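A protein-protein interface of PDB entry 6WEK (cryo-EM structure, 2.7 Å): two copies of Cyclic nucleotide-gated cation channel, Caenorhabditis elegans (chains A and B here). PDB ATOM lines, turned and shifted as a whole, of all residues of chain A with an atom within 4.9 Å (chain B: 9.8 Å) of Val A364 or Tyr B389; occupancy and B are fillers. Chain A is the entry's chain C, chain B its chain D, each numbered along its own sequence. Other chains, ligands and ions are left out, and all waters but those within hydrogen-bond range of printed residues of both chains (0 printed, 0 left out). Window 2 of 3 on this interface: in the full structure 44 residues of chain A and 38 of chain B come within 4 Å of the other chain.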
ATOM      1  N   GLN A 349      37.639  18.795 -29.427  1.00  0.00           N
ATOM      2  CA  GLN A 349      36.800  17.693 -28.999  1.00  0.00           C
ATOM      3  C   GLN A 349      35.540  18.199 -28.338  1.00  0.00           C
ATOM      4  O   GLN A 349      34.496  17.549 -28.427  1.00  0.00           O
ATOM      5  CB  GLN A 349      37.560  16.779 -28.040  1.00  0.00           C
ATOM      6  CG  GLN A 349      36.702  15.713 -27.416  1.00  0.00           C
ATOM      7  CD  GLN A 349      37.502  14.681 -26.689  1.00  0.00           C
ATOM      8  OE1 GLN A 349      38.679  14.510 -26.951  1.00  0.00           O
ATOM      9  NE2 GLN A 349      36.873  13.981 -25.773  1.00  0.00           N
ATOM     10  N   SER A 350      35.621  19.355 -27.687  1.00  0.00           N
ATOM     11  CA  SER A 350      34.442  20.009 -27.148  1.00  0.00           C
ATOM     12  C   SER A 350      33.646  20.678 -28.250  1.00  0.00           C
ATOM     13  O   SER A 350      32.417  20.585 -28.273  1.00  0.00           O
ATOM     14  CB  SER A 350      34.847  21.031 -26.095  1.00  0.00           C
ATOM     15  OG  SER A 350      35.548  22.098 -26.689  1.00  0.00           O
ATOM     16  N   LEU A 360      23.818  23.668 -23.407  1.00  0.00           N
ATOM     17  CA  LEU A 360      23.742  22.215 -23.340  1.00  0.00           C
ATOM     18  C   LEU A 360      25.067  21.580 -23.723  1.00  0.00           C
ATOM     19  O   LEU A 360      25.469  20.575 -23.135  1.00  0.00           O
ATOM     20  CB  LEU A 360      22.626  21.705 -24.244  1.00  0.00           C
ATOM     21  CG  LEU A 360      22.396  20.198 -24.310  1.00  0.00           C
ATOM     22  CD1 LEU A 360      22.034  19.647 -22.964  1.00  0.00           C
ATOM     23  CD2 LEU A 360      21.316  19.902 -25.295  1.00  0.00           C
ATOM     24  N   ARG A 361      25.762  22.150 -24.704  1.00  0.00           N
ATOM     25  CA  ARG A 361      27.053  21.615 -25.107  1.00  0.00           C
ATOM     26  C   ARG A 361      28.077  21.746 -23.990  1.00  0.00           C
ATOM     27  O   ARG A 361      28.874  20.832 -23.763  1.00  0.00           O
ATOM     28  CB  ARG A 361      27.533  22.331 -26.360  1.00  0.00           C
ATOM     29  CG  ARG A 361      28.811  21.805 -26.933  1.00  0.00           C
ATOM     30  CD  ARG A 361      28.647  20.379 -27.335  1.00  0.00           C
ATOM     31  NE  ARG A 361      29.807  19.871 -28.046  1.00  0.00           N
ATOM     32  CZ  ARG A 361      29.897  18.636 -28.510  1.00  0.00           C
ATOM     33  NH1 ARG A 361      28.899  17.799 -28.329  1.00  0.00           N
ATOM     34  NH2 ARG A 361      30.979  18.240 -29.148  1.00  0.00           N
ATOM     35  N   ARG A 362      28.062  22.871 -23.274  1.00  0.00           N
ATOM     36  CA  ARG A 362      29.028  23.089 -22.202  1.00  0.00           C
ATOM     37  C   ARG A 362      28.859  22.078 -21.086  1.00  0.00           C
ATOM     38  O   ARG A 362      29.844  21.647 -20.484  1.00  0.00           O
ATOM     39  CB  ARG A 362      28.886  24.500 -21.653  1.00  0.00           C
ATOM     40  CG  ARG A 362      29.071  25.539 -22.692  1.00  0.00           C
ATOM     41  CD  ARG A 362      29.048  26.906 -22.120  1.00  0.00           C
ATOM     42  NE  ARG A 362      29.596  27.852 -23.073  1.00  0.00           N
ATOM     43  CZ  ARG A 362      30.010  29.069 -22.759  1.00  0.00           C
ATOM     44  NH1 ARG A 362      29.935  29.487 -21.513  1.00  0.00           N
ATOM     45  NH2 ARG A 362      30.503  29.860 -23.691  1.00  0.00           N
ATOM     46  N   TYR A 363      27.624  21.698 -20.782  1.00  0.00           N
ATOM     47  CA  TYR A 363      27.415  20.718 -19.730  1.00  0.00           C
ATOM     48  C   TYR A 363      27.622  19.302 -20.236  1.00  0.00           C
ATOM     49  O   TYR A 363      28.121  18.450 -19.499  1.00  0.00           O
ATOM     50  CB  TYR A 363      26.025  20.864 -19.124  1.00  0.00           C
ATOM     51  CG  TYR A 363      25.820  19.903 -17.989  1.00  0.00           C
ATOM     52  CD1 TYR A 363      26.407  20.127 -16.763  1.00  0.00           C
ATOM     53  CD2 TYR A 363      25.072  18.756 -18.150  1.00  0.00           C
ATOM     54  CE1 TYR A 363      26.248  19.253 -15.735  1.00  0.00           C
ATOM     55  CE2 TYR A 363      24.909  17.877 -17.124  1.00  0.00           C
ATOM     56  CZ  TYR A 363      25.498  18.133 -15.921  1.00  0.00           C
ATOM     57  OH  TYR A 363      25.343  17.261 -14.882  1.00  0.00           O
ATOM     58  N   VAL A 364      27.264  19.032 -21.486  1.00  0.00           N
ATOM     59  CA  VAL A 364      27.427  17.690 -22.029  1.00  0.00           C
ATOM     60  C   VAL A 364      28.902  17.336 -22.138  1.00  0.00           C
ATOM     61  O   VAL A 364      29.333  16.261 -21.701  1.00  0.00           O
ATOM     62  CB  VAL A 364      26.703  17.586 -23.383  1.00  0.00           C
ATOM     63  CG1 VAL A 364      27.261  16.473 -24.207  1.00  0.00           C
ATOM     64  CG2 VAL A 364      25.234  17.368 -23.161  1.00  0.00           C
ATOM     65  N   TYR A 365      29.708  18.243 -22.688  1.00  0.00           N
ATOM     66  CA  TYR A 365      31.130  17.963 -22.790  1.00  0.00           C
ATOM     67  C   TYR A 365      31.796  17.891 -21.427  1.00  0.00           C
ATOM     68  O   TYR A 365      32.718  17.099 -21.238  1.00  0.00           O
ATOM     69  CB  TYR A 365      31.828  19.007 -23.642  1.00  0.00           C
ATOM     70  CG  TYR A 365      33.302  18.748 -23.723  1.00  0.00           C
ATOM     71  CD1 TYR A 365      33.797  17.740 -24.521  1.00  0.00           C
ATOM     72  CD2 TYR A 365      34.198  19.489 -22.976  1.00  0.00           C
ATOM     73  CE1 TYR A 365      35.135  17.488 -24.586  1.00  0.00           C
ATOM     74  CE2 TYR A 365      35.538  19.241 -23.038  1.00  0.00           C
ATOM     75  CZ  TYR A 365      36.000  18.237 -23.846  1.00  0.00           C
ATOM     76  OH  TYR A 365      37.341  17.983 -23.918  1.00  0.00           O
ATOM     77  N   SER A 366      31.349  18.688 -20.462  1.00  0.00           N
ATOM     78  CA  SER A 366      31.965  18.654 -19.143  1.00  0.00           C
ATOM     79  C   SER A 366      31.624  17.370 -18.407  1.00  0.00           C
ATOM     80  O   SER A 366      32.481  16.789 -17.737  1.00  0.00           O
ATOM     81  CB  SER A 366      31.529  19.869 -18.344  1.00  0.00           C
ATOM     82  OG  SER A 366      31.678  21.037 -19.116  1.00  0.00           O
ATOM     83  N   PHE A 367      30.380  16.907 -18.521  1.00  0.00           N
ATOM     84  CA  PHE A 367      30.001  15.629 -17.934  1.00  0.00           C
ATOM     85  C   PHE A 367      30.772  14.483 -18.575  1.00  0.00           C
ATOM     86  O   PHE A 367      31.208  13.555 -17.888  1.00  0.00           O
ATOM     87  CB  PHE A 367      28.496  15.425 -18.083  1.00  0.00           C
ATOM     88  CG  PHE A 367      27.917  14.427 -17.132  1.00  0.00           C
ATOM     89  CD1 PHE A 367      27.882  13.091 -17.448  1.00  0.00           C
ATOM     90  CD2 PHE A 367      27.395  14.830 -15.930  1.00  0.00           C
ATOM     91  CE1 PHE A 367      27.355  12.185 -16.581  1.00  0.00           C
ATOM     92  CE2 PHE A 367      26.865  13.923 -15.063  1.00  0.00           C
ATOM     93  CZ  PHE A 367      26.846  12.601 -15.388  1.00  0.00           C
ATOM     94  N   TYR A 368      30.978  14.544 -19.891  1.00  0.00           N
ATOM     95  CA  TYR A 368      31.768  13.520 -20.562  1.00  0.00           C
ATOM     96  C   TYR A 368      33.224  13.547 -20.111  1.00  0.00           C
ATOM     97  O   TYR A 368      33.823  12.496 -19.852  1.00  0.00           O
ATOM     98  CB  TYR A 368      31.666  13.717 -22.068  1.00  0.00           C
ATOM     99  CG  TYR A 368      32.494  12.771 -22.887  1.00  0.00           C
ATOM    100  CD1 TYR A 368      32.106  11.458 -23.069  1.00  0.00           C
ATOM    101  CD2 TYR A 368      33.657  13.198 -23.501  1.00  0.00           C
ATOM    102  CE1 TYR A 368      32.853  10.602 -23.823  1.00  0.00           C
ATOM    103  CE2 TYR A 368      34.405  12.350 -24.258  1.00  0.00           C
ATOM    104  CZ  TYR A 368      34.002  11.056 -24.416  1.00  0.00           C
ATOM    105  OH  TYR A 368      34.760  10.207 -25.176  1.00  0.00           O
ATOM    106  N   ILE B 330      22.182   2.740 -33.589  1.00  0.00           N
ATOM    107  CA  ILE B 330      22.291   4.178 -33.383  1.00  0.00           C
ATOM    108  C   ILE B 330      23.046   4.830 -34.528  1.00  0.00           C
ATOM    109  O   ILE B 330      22.716   5.939 -34.948  1.00  0.00           O
ATOM    110  CB  ILE B 330      22.950   4.473 -32.030  1.00  0.00           C
ATOM    111  CG1 ILE B 330      22.126   3.844 -30.925  1.00  0.00           C
ATOM    112  CG2 ILE B 330      23.045   5.954 -31.804  1.00  0.00           C
ATOM    113  CD1 ILE B 330      22.419   4.373 -29.580  1.00  0.00           C
ATOM    114  N   ILE B 334      21.225   7.705 -36.717  1.00  0.00           N
ATOM    115  CA  ILE B 334      21.869   8.997 -36.911  1.00  0.00           C
ATOM    116  C   ILE B 334      22.205   9.203 -38.377  1.00  0.00           C
ATOM    117  O   ILE B 334      22.040  10.298 -38.921  1.00  0.00           O
ATOM    118  CB  ILE B 334      23.120   9.097 -36.022  1.00  0.00           C
ATOM    119  CG1 ILE B 334      22.716   9.130 -34.558  1.00  0.00           C
ATOM    120  CG2 ILE B 334      23.925  10.312 -36.358  1.00  0.00           C
ATOM    121  CD1 ILE B 334      23.863   9.046 -33.630  1.00  0.00           C
ATOM    122  N   ASP B 339      29.199  11.667 -39.351  1.00  0.00           N
ATOM    123  CA  ASP B 339      30.277  12.232 -38.555  1.00  0.00           C
ATOM    124  C   ASP B 339      31.357  11.164 -38.417  1.00  0.00           C
ATOM    125  O   ASP B 339      31.344  10.135 -39.096  1.00  0.00           O
ATOM    126  CB  ASP B 339      29.754  12.758 -37.214  1.00  0.00           C
ATOM    127  CG  ASP B 339      28.973  11.737 -36.452  1.00  0.00           C
ATOM    128  OD1 ASP B 339      29.534  10.683 -36.132  1.00  0.00           O
ATOM    129  OD2 ASP B 339      27.797  11.997 -36.157  1.00  0.00           O
ATOM    130  N   TRP B 341      32.184   9.523 -35.552  1.00  0.00           N
ATOM    131  CA  TRP B 341      31.896   8.531 -34.530  1.00  0.00           C
ATOM    132  C   TRP B 341      31.020   7.418 -35.051  1.00  0.00           C
ATOM    133  O   TRP B 341      31.120   6.284 -34.585  1.00  0.00           O
ATOM    134  CB  TRP B 341      31.203   9.199 -33.340  1.00  0.00           C
ATOM    135  CG  TRP B 341      30.783   8.293 -32.248  1.00  0.00           C
ATOM    136  CD1 TRP B 341      31.494   7.966 -31.152  1.00  0.00           C
ATOM    137  CD2 TRP B 341      29.529   7.623 -32.125  1.00  0.00           C
ATOM    138  NE1 TRP B 341      30.779   7.123 -30.356  1.00  0.00           N
ATOM    139  CE2 TRP B 341      29.562   6.899 -30.934  1.00  0.00           C
ATOM    140  CE3 TRP B 341      28.382   7.558 -32.917  1.00  0.00           C
ATOM    141  CZ2 TRP B 341      28.502   6.120 -30.515  1.00  0.00           C
ATOM    142  CZ3 TRP B 341      27.338   6.787 -32.500  1.00  0.00           C
ATOM    143  CH2 TRP B 341      27.401   6.080 -31.313  1.00  0.00           C
ATOM    144  N   TRP B 369      34.088  -2.265 -31.395  1.00  0.00           N
ATOM    145  CA  TRP B 369      33.724  -1.048 -30.686  1.00  0.00           C
ATOM    146  C   TRP B 369      33.106  -1.365 -29.333  1.00  0.00           C
ATOM    147  O   TRP B 369      33.459  -0.758 -28.318  1.00  0.00           O
ATOM    148  CB  TRP B 369      32.765  -0.233 -31.548  1.00  0.00           C
ATOM    149  CG  TRP B 369      32.524   1.156 -31.089  1.00  0.00           C
ATOM    150  CD1 TRP B 369      33.151   2.271 -31.521  1.00  0.00           C
ATOM    151  CD2 TRP B 369      31.565   1.583 -30.122  1.00  0.00           C
ATOM    152  NE1 TRP B 369      32.656   3.370 -30.883  1.00  0.00           N
ATOM    153  CE2 TRP B 369      31.678   2.970 -30.014  1.00  0.00           C
ATOM    154  CE3 TRP B 369      30.624   0.924 -29.334  1.00  0.00           C
ATOM    155  CZ2 TRP B 369      30.891   3.708 -29.153  1.00  0.00           C
ATOM    156  CZ3 TRP B 369      29.849   1.655 -28.486  1.00  0.00           C
ATOM    157  CH2 TRP B 369      29.985   3.033 -28.399  1.00  0.00           C
ATOM    158  N   ILE B 373      34.461  -0.405 -25.594  1.00  0.00           N
ATOM    159  CA  ILE B 373      33.682   0.489 -24.744  1.00  0.00           C
ATOM    160  C   ILE B 373      33.273  -0.203 -23.453  1.00  0.00           C
ATOM    161  O   ILE B 373      33.370   0.376 -22.369  1.00  0.00           O
ATOM    162  CB  ILE B 373      32.468   1.029 -25.510  1.00  0.00           C
ATOM    163  CG1 ILE B 373      32.926   2.046 -26.541  1.00  0.00           C
ATOM    164  CG2 ILE B 373      31.500   1.674 -24.573  1.00  0.00           C
ATOM    165  CD1 ILE B 373      33.481   3.290 -25.955  1.00  0.00           C
ATOM    166  N   PRO B 381      36.892   6.260 -31.757  1.00  0.00           N
ATOM    167  CA  PRO B 381      36.661   7.690 -31.974  1.00  0.00           C
ATOM    168  C   PRO B 381      35.724   8.282 -30.935  1.00  0.00           C
ATOM    169  O   PRO B 381      34.895   7.590 -30.345  1.00  0.00           O
ATOM    170  CB  PRO B 381      36.051   7.733 -33.374  1.00  0.00           C
ATOM    171  CG  PRO B 381      36.648   6.589 -34.036  1.00  0.00           C
ATOM    172  CD  PRO B 381      36.742   5.510 -33.011  1.00  0.00           C
ATOM    173  N   SER B 382      35.873   9.562 -30.702  1.00  0.00           N
ATOM    174  CA  SER B 382      35.107  10.230 -29.669  1.00  0.00           C
ATOM    175  C   SER B 382      33.809  10.774 -30.239  1.00  0.00           C
ATOM    176  O   SER B 382      33.723  11.059 -31.435  1.00  0.00           O
ATOM    177  CB  SER B 382      35.932  11.356 -29.057  1.00  0.00           C
ATOM    178  OG  SER B 382      36.635  12.066 -30.051  1.00  0.00           O
ATOM    179  N   PRO B 383      32.778  10.920 -29.408  1.00  0.00           N
ATOM    180  CA  PRO B 383      31.478  11.350 -29.919  1.00  0.00           C
ATOM    181  C   PRO B 383      31.542  12.751 -30.498  1.00  0.00           C
ATOM    182  O   PRO B 383      32.390  13.559 -30.124  1.00  0.00           O
ATOM    183  CB  PRO B 383      30.585  11.300 -28.681  1.00  0.00           C
ATOM    184  CG  PRO B 383      31.285  10.433 -27.741  1.00  0.00           C
ATOM    185  CD  PRO B 383      32.718  10.629 -27.972  1.00  0.00           C
ATOM    186  N   VAL B 384      30.644  13.031 -31.433  1.00  0.00           N
ATOM    187  CA  VAL B 384      30.656  14.318 -32.112  1.00  0.00           C
ATOM    188  C   VAL B 384      29.411  15.114 -31.764  1.00  0.00           C
ATOM    189  O   VAL B 384      29.443  16.346 -31.727  1.00  0.00           O
ATOM    190  CB  VAL B 384      30.785  14.132 -33.629  1.00  0.00           C
ATOM    191  CG1 VAL B 384      30.920  15.460 -34.307  1.00  0.00           C
ATOM    192  CG2 VAL B 384      31.974  13.269 -33.943  1.00  0.00           C
ATOM    193  N   ARG B 385      28.317  14.426 -31.483  1.00  0.00           N
ATOM    194  CA  ARG B 385      27.034  15.061 -31.256  1.00  0.00           C
ATOM    195  C   ARG B 385      26.557  14.790 -29.841  1.00  0.00           C
ATOM    196  O   ARG B 385      27.016  13.865 -29.177  1.00  0.00           O
ATOM    197  CB  ARG B 385      26.003  14.568 -32.257  1.00  0.00           C
ATOM    198  CG  ARG B 385      26.432  14.785 -33.665  1.00  0.00           C
ATOM    199  CD  ARG B 385      25.451  14.191 -34.612  1.00  0.00           C
ATOM    200  NE  ARG B 385      24.137  14.785 -34.458  1.00  0.00           N
ATOM    201  CZ  ARG B 385      23.202  14.746 -35.392  1.00  0.00           C
ATOM    202  NH1 ARG B 385      23.449  14.144 -36.543  1.00  0.00           N
ATOM    203  NH2 ARG B 385      22.027  15.312 -35.181  1.00  0.00           N
ATOM    204  N   ASN B 386      25.622  15.617 -29.384  1.00  0.00           N
ATOM    205  CA  ASN B 386      25.120  15.486 -28.023  1.00  0.00           C
ATOM    206  C   ASN B 386      24.483  14.128 -27.795  1.00  0.00           C
ATOM    207  O   ASN B 386      24.636  13.546 -26.718  1.00  0.00           O
ATOM    208  CB  ASN B 386      24.108  16.588 -27.728  1.00  0.00           C
ATOM    209  CG  ASN B 386      24.737  17.951 -27.638  1.00  0.00           C
ATOM    210  OD1 ASN B 386      24.512  18.672 -26.684  1.00  0.00           O
ATOM    211  ND2 ASN B 386      25.522  18.315 -28.631  1.00  0.00           N
ATOM    212  N   ILE B 387      23.769  13.610 -28.790  1.00  0.00           N
ATOM    213  CA  ILE B 387      23.130  12.307 -28.646  1.00  0.00           C
ATOM    214  C   ILE B 387      24.182  11.210 -28.539  1.00  0.00           C
ATOM    215  O   ILE B 387      24.033  10.258 -27.765  1.00  0.00           O
ATOM    216  CB  ILE B 387      22.144  12.073 -29.807  1.00  0.00           C
ATOM    217  CG1 ILE B 387      21.294  10.838 -29.549  1.00  0.00           C
ATOM    218  CG2 ILE B 387      22.855  11.980 -31.136  1.00  0.00           C
ATOM    219  CD1 ILE B 387      20.430  10.965 -28.337  1.00  0.00           C
ATOM    220  N   GLU B 388      25.281  11.347 -29.282  1.00  0.00           N
ATOM    221  CA  GLU B 388      26.363  10.376 -29.198  1.00  0.00           C
ATOM    222  C   GLU B 388      27.104  10.489 -27.877  1.00  0.00           C
ATOM    223  O   GLU B 388      27.549   9.482 -27.329  1.00  0.00           O
ATOM    224  CB  GLU B 388      27.319  10.567 -30.359  1.00  0.00           C
ATOM    225  CG  GLU B 388      26.660  10.441 -31.685  1.00  0.00           C
ATOM    226  CD  GLU B 388      27.560  10.865 -32.786  1.00  0.00           C
ATOM    227  OE1 GLU B 388      28.662  11.325 -32.480  1.00  0.00           O
ATOM    228  OE2 GLU B 388      27.180  10.743 -33.956  1.00  0.00           O
ATOM    229  N   TYR B 389      27.242  11.701 -27.347  1.00  0.00           N
ATOM    230  CA  TYR B 389      27.821  11.860 -26.021  1.00  0.00           C
ATOM    231  C   TYR B 389      26.973  11.174 -24.968  1.00  0.00           C
ATOM    232  O   TYR B 389      27.498  10.479 -24.098  1.00  0.00           O
ATOM    233  CB  TYR B 389      27.974  13.336 -25.683  1.00  0.00           C
ATOM    234  CG  TYR B 389      29.272  13.926 -26.132  1.00  0.00           C
ATOM    235  CD1 TYR B 389      29.406  14.461 -27.383  1.00  0.00           C
ATOM    236  CD2 TYR B 389      30.362  13.949 -25.302  1.00  0.00           C
ATOM    237  CE1 TYR B 389      30.583  14.994 -27.793  1.00  0.00           C
ATOM    238  CE2 TYR B 389      31.541  14.482 -25.707  1.00  0.00           C
ATOM    239  CZ  TYR B 389      31.649  15.001 -26.954  1.00  0.00           C
ATOM    240  OH  TYR B 389      32.835  15.536 -27.369  1.00  0.00           O
ATOM    241  N   ALA B 390      25.657  11.368 -25.027  1.00  0.00           N
ATOM    242  CA  ALA B 390      24.771  10.710 -24.078  1.00  0.00           C
ATOM    243  C   ALA B 390      24.868   9.196 -24.189  1.00  0.00           C
ATOM    244  O   ALA B 390      24.990   8.497 -23.174  1.00  0.00           O
ATOM    245  CB  ALA B 390      23.338  11.172 -24.304  1.00  0.00           C
ATOM    246  N   PHE B 391      24.837   8.676 -25.418  1.00  0.00           N
ATOM    247  CA  PHE B 391      24.936   7.236 -25.619  1.00  0.00           C
ATOM    248  C   PHE B 391      26.246   6.686 -25.078  1.00  0.00           C
ATOM    249  O   PHE B 391      26.252   5.696 -24.346  1.00  0.00           O
ATOM    250  CB  PHE B 391      24.789   6.893 -27.097  1.00  0.00           C
ATOM    251  CG  PHE B 391      25.073   5.456 -27.411  1.00  0.00           C
ATOM    252  CD1 PHE B 391      24.350   4.445 -26.811  1.00  0.00           C
ATOM    253  CD2 PHE B 391      26.065   5.112 -28.306  1.00  0.00           C
ATOM    254  CE1 PHE B 391      24.615   3.125 -27.101  1.00  0.00           C
ATOM    255  CE2 PHE B 391      26.325   3.795 -28.590  1.00  0.00           C
ATOM    256  CZ  PHE B 391      25.603   2.805 -27.989  1.00  0.00           C
ATOM    257  N   VAL B 392      27.369   7.315 -25.424  1.00  0.00           N
ATOM    258  CA  VAL B 392      28.665   6.785 -25.023  1.00  0.00           C
ATOM    259  C   VAL B 392      28.872   6.918 -23.522  1.00  0.00           C
ATOM    260  O   VAL B 392      29.483   6.051 -22.899  1.00  0.00           O
ATOM    261  CB  VAL B 392      29.789   7.467 -25.813  1.00  0.00           C
ATOM    262  CG1 VAL B 392      31.122   6.992 -25.328  1.00  0.00           C
ATOM    263  CG2 VAL B 392      29.650   7.147 -27.259  1.00  0.00           C
ATOM    264  N   THR B 393      28.371   7.988 -22.908  1.00  0.00           N
ATOM    265  CA  THR B 393      28.500   8.126 -21.462  1.00  0.00           C
ATOM    266  C   THR B 393      27.708   7.044 -20.744  1.00  0.00           C
ATOM    267  O   THR B 393      28.224   6.369 -19.843  1.00  0.00           O
ATOM    268  CB  THR B 393      28.035   9.510 -21.030  1.00  0.00           C
ATOM    269  OG1 THR B 393      28.722  10.499 -21.795  1.00  0.00           O
ATOM    270  CG2 THR B 393      28.334   9.737 -19.580  1.00  0.00           C
ATOM    271  N   LEU B 394      26.447   6.862 -21.138  1.00  0.00           N
ATOM    272  CA  LEU B 394      25.638   5.805 -20.549  1.00  0.00           C
ATOM    273  C   LEU B 394      26.266   4.439 -20.780  1.00  0.00           C
ATOM    274  O   LEU B 394      26.266   3.586 -19.887  1.00  0.00           O
ATOM    275  CB  LEU B 394      24.236   5.862 -21.135  1.00  0.00           C
ATOM    276  CG  LEU B 394      23.209   4.881 -20.595  1.00  0.00           C
ATOM    277  CD1 LEU B 394      22.967   5.129 -19.123  1.00  0.00           C
ATOM    278  CD2 LEU B 394      21.931   5.024 -21.382  1.00  0.00           C
ATOM    279  N   ASP B 395      26.832   4.228 -21.967  1.00  0.00           N
ATOM    280  CA  ASP B 395      27.423   2.942 -22.309  1.00  0.00           C
ATOM    281  C   ASP B 395      28.695   2.681 -21.520  1.00  0.00           C
ATOM    282  O   ASP B 395      28.934   1.555 -21.088  1.00  0.00           O
ATOM    283  CB  ASP B 395      27.699   2.897 -23.805  1.00  0.00           C
ATOM    284  CG  ASP B 395      27.609   1.516 -24.359  1.00  0.00           C
ATOM    285  OD1 ASP B 395      27.096   0.637 -23.653  1.00  0.00           O
ATOM    286  OD2 ASP B 395      28.052   1.301 -25.498  1.00  0.00           O
ATOM    287  N   LEU B 396      29.603   3.604 -21.362  1.00  0.00           N
ATOM    288  CA  LEU B 396      30.783   3.432 -20.567  1.00  0.00           C
ATOM    289  C   LEU B 396      30.485   3.213 -19.168  1.00  0.00           C
ATOM    290  O   LEU B 396      31.242   2.710 -18.517  1.00  0.00           O
ATOM    291  CB  LEU B 396      31.666   4.594 -20.600  1.00  0.00           C
ATOM    292  CG  LEU B 396      32.435   4.899 -21.801  1.00  0.00           C
ATOM    293  CD1 LEU B 396      32.769   6.313 -21.697  1.00  0.00           C
ATOM    294  CD2 LEU B 396      33.689   4.150 -21.915  1.00  0.00           C
ATOM    295  N   MET B 397      29.488   3.815 -18.625  1.00  0.00           N
ATOM    296  CA  MET B 397      29.083   3.601 -17.287  1.00  0.00           C
ATOM    297  C   MET B 397      28.529   2.267 -17.086  1.00  0.00           C
ATOM    298  O   MET B 397      28.821   1.671 -16.164  1.00  0.00           O
ATOM    299  CB  MET B 397      28.139   4.635 -16.866  1.00  0.00           C
ATOM    300  CG  MET B 397      28.802   5.751 -16.093  1.00  0.00           C
ATOM    301  SD  MET B 397      30.240   5.516 -15.024  1.00  0.00           S
ATOM    302  CE  MET B 397      29.797   4.532 -13.677  1.00  0.00           C
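Hydrophobic or aromatic side chains of chain A that line the printed part of chain B: Leu A360, Val A364, Tyr A365, Phe A367 and Tyr A368. Of the 23 printed residues of chain B, 5 touch a printed residue of chain A. Hydrophobic or aromatic side chains of chain B within 4 Å of the printed part of chain A: Pro B383 and Tyr B389.
Among the printed residues, pairs that only touch across the chains: Arg A361 with Tyr B389 (3.3 Å), Tyr A368 with Tyr B389 (3.3 Å), Tyr A368 with Pro B383 (3.5 Å), Leu A360 with Asn B386 (3.5 Å), Val A364 with Tyr B389 (3.5 Å), Arg A361 with Val B384 (3.5 Å), Tyr A365 with Tyr B389 (3.7 Å), Tyr A368 with Thr B393 (3.7 Å), Val A364 with Asn B386 (3.8 Å) and Phe A367 with Thr B393 (3.99 Å).
Val A364 touches just these residues of chain B: Asn B386 and Tyr B389. Tyr B389 touches five residues of chain A. No residue of chain B comes within 4 Å of Ser A366. Of the printed residues of chain B, Arg A361 touches Val B384, Asn B386 and Tyr B389. Of the printed residues of chain B, Gln A349 touches Tyr B389 (2.8 Å). Tyr A363 touches none of the printed residues of chain B. Asp B395 touches none of the printed residues of chain A. The nearest residue of chain A that does not touch Tyr B389 is Ser A350 (4.7 Å). The nearest printed residue of chain B that does not touch Leu A360 is Ile B387 (7.6 Å).
The side-chain hydroxyl of Tyr B389 lies within hydrogen-bond range of the backbone carbonyl oxygen of Gln A349 (2.8 Å). The side-chain amide nitrogen (ND2) of Asn B386 lies close to the guanidinium group (NH1) of Arg A361 (3.4 Å).
NE of Arg A361 lies within hydrogen-bond range of O of Ser A350. The side-chain hydroxyl (OH) of Tyr B389 sits close to the backbone carbonyl oxygen (O) of Pro B383, 3.4 Å away. The side-chain carboxylate of Glu B388 is in hydrogen-bond range of the backbone NH of Val B384 (2.8 Å). O of Tyr B389 lies within hydrogen-bond range of OG1 of Thr B393.
No position is printed for both chains.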
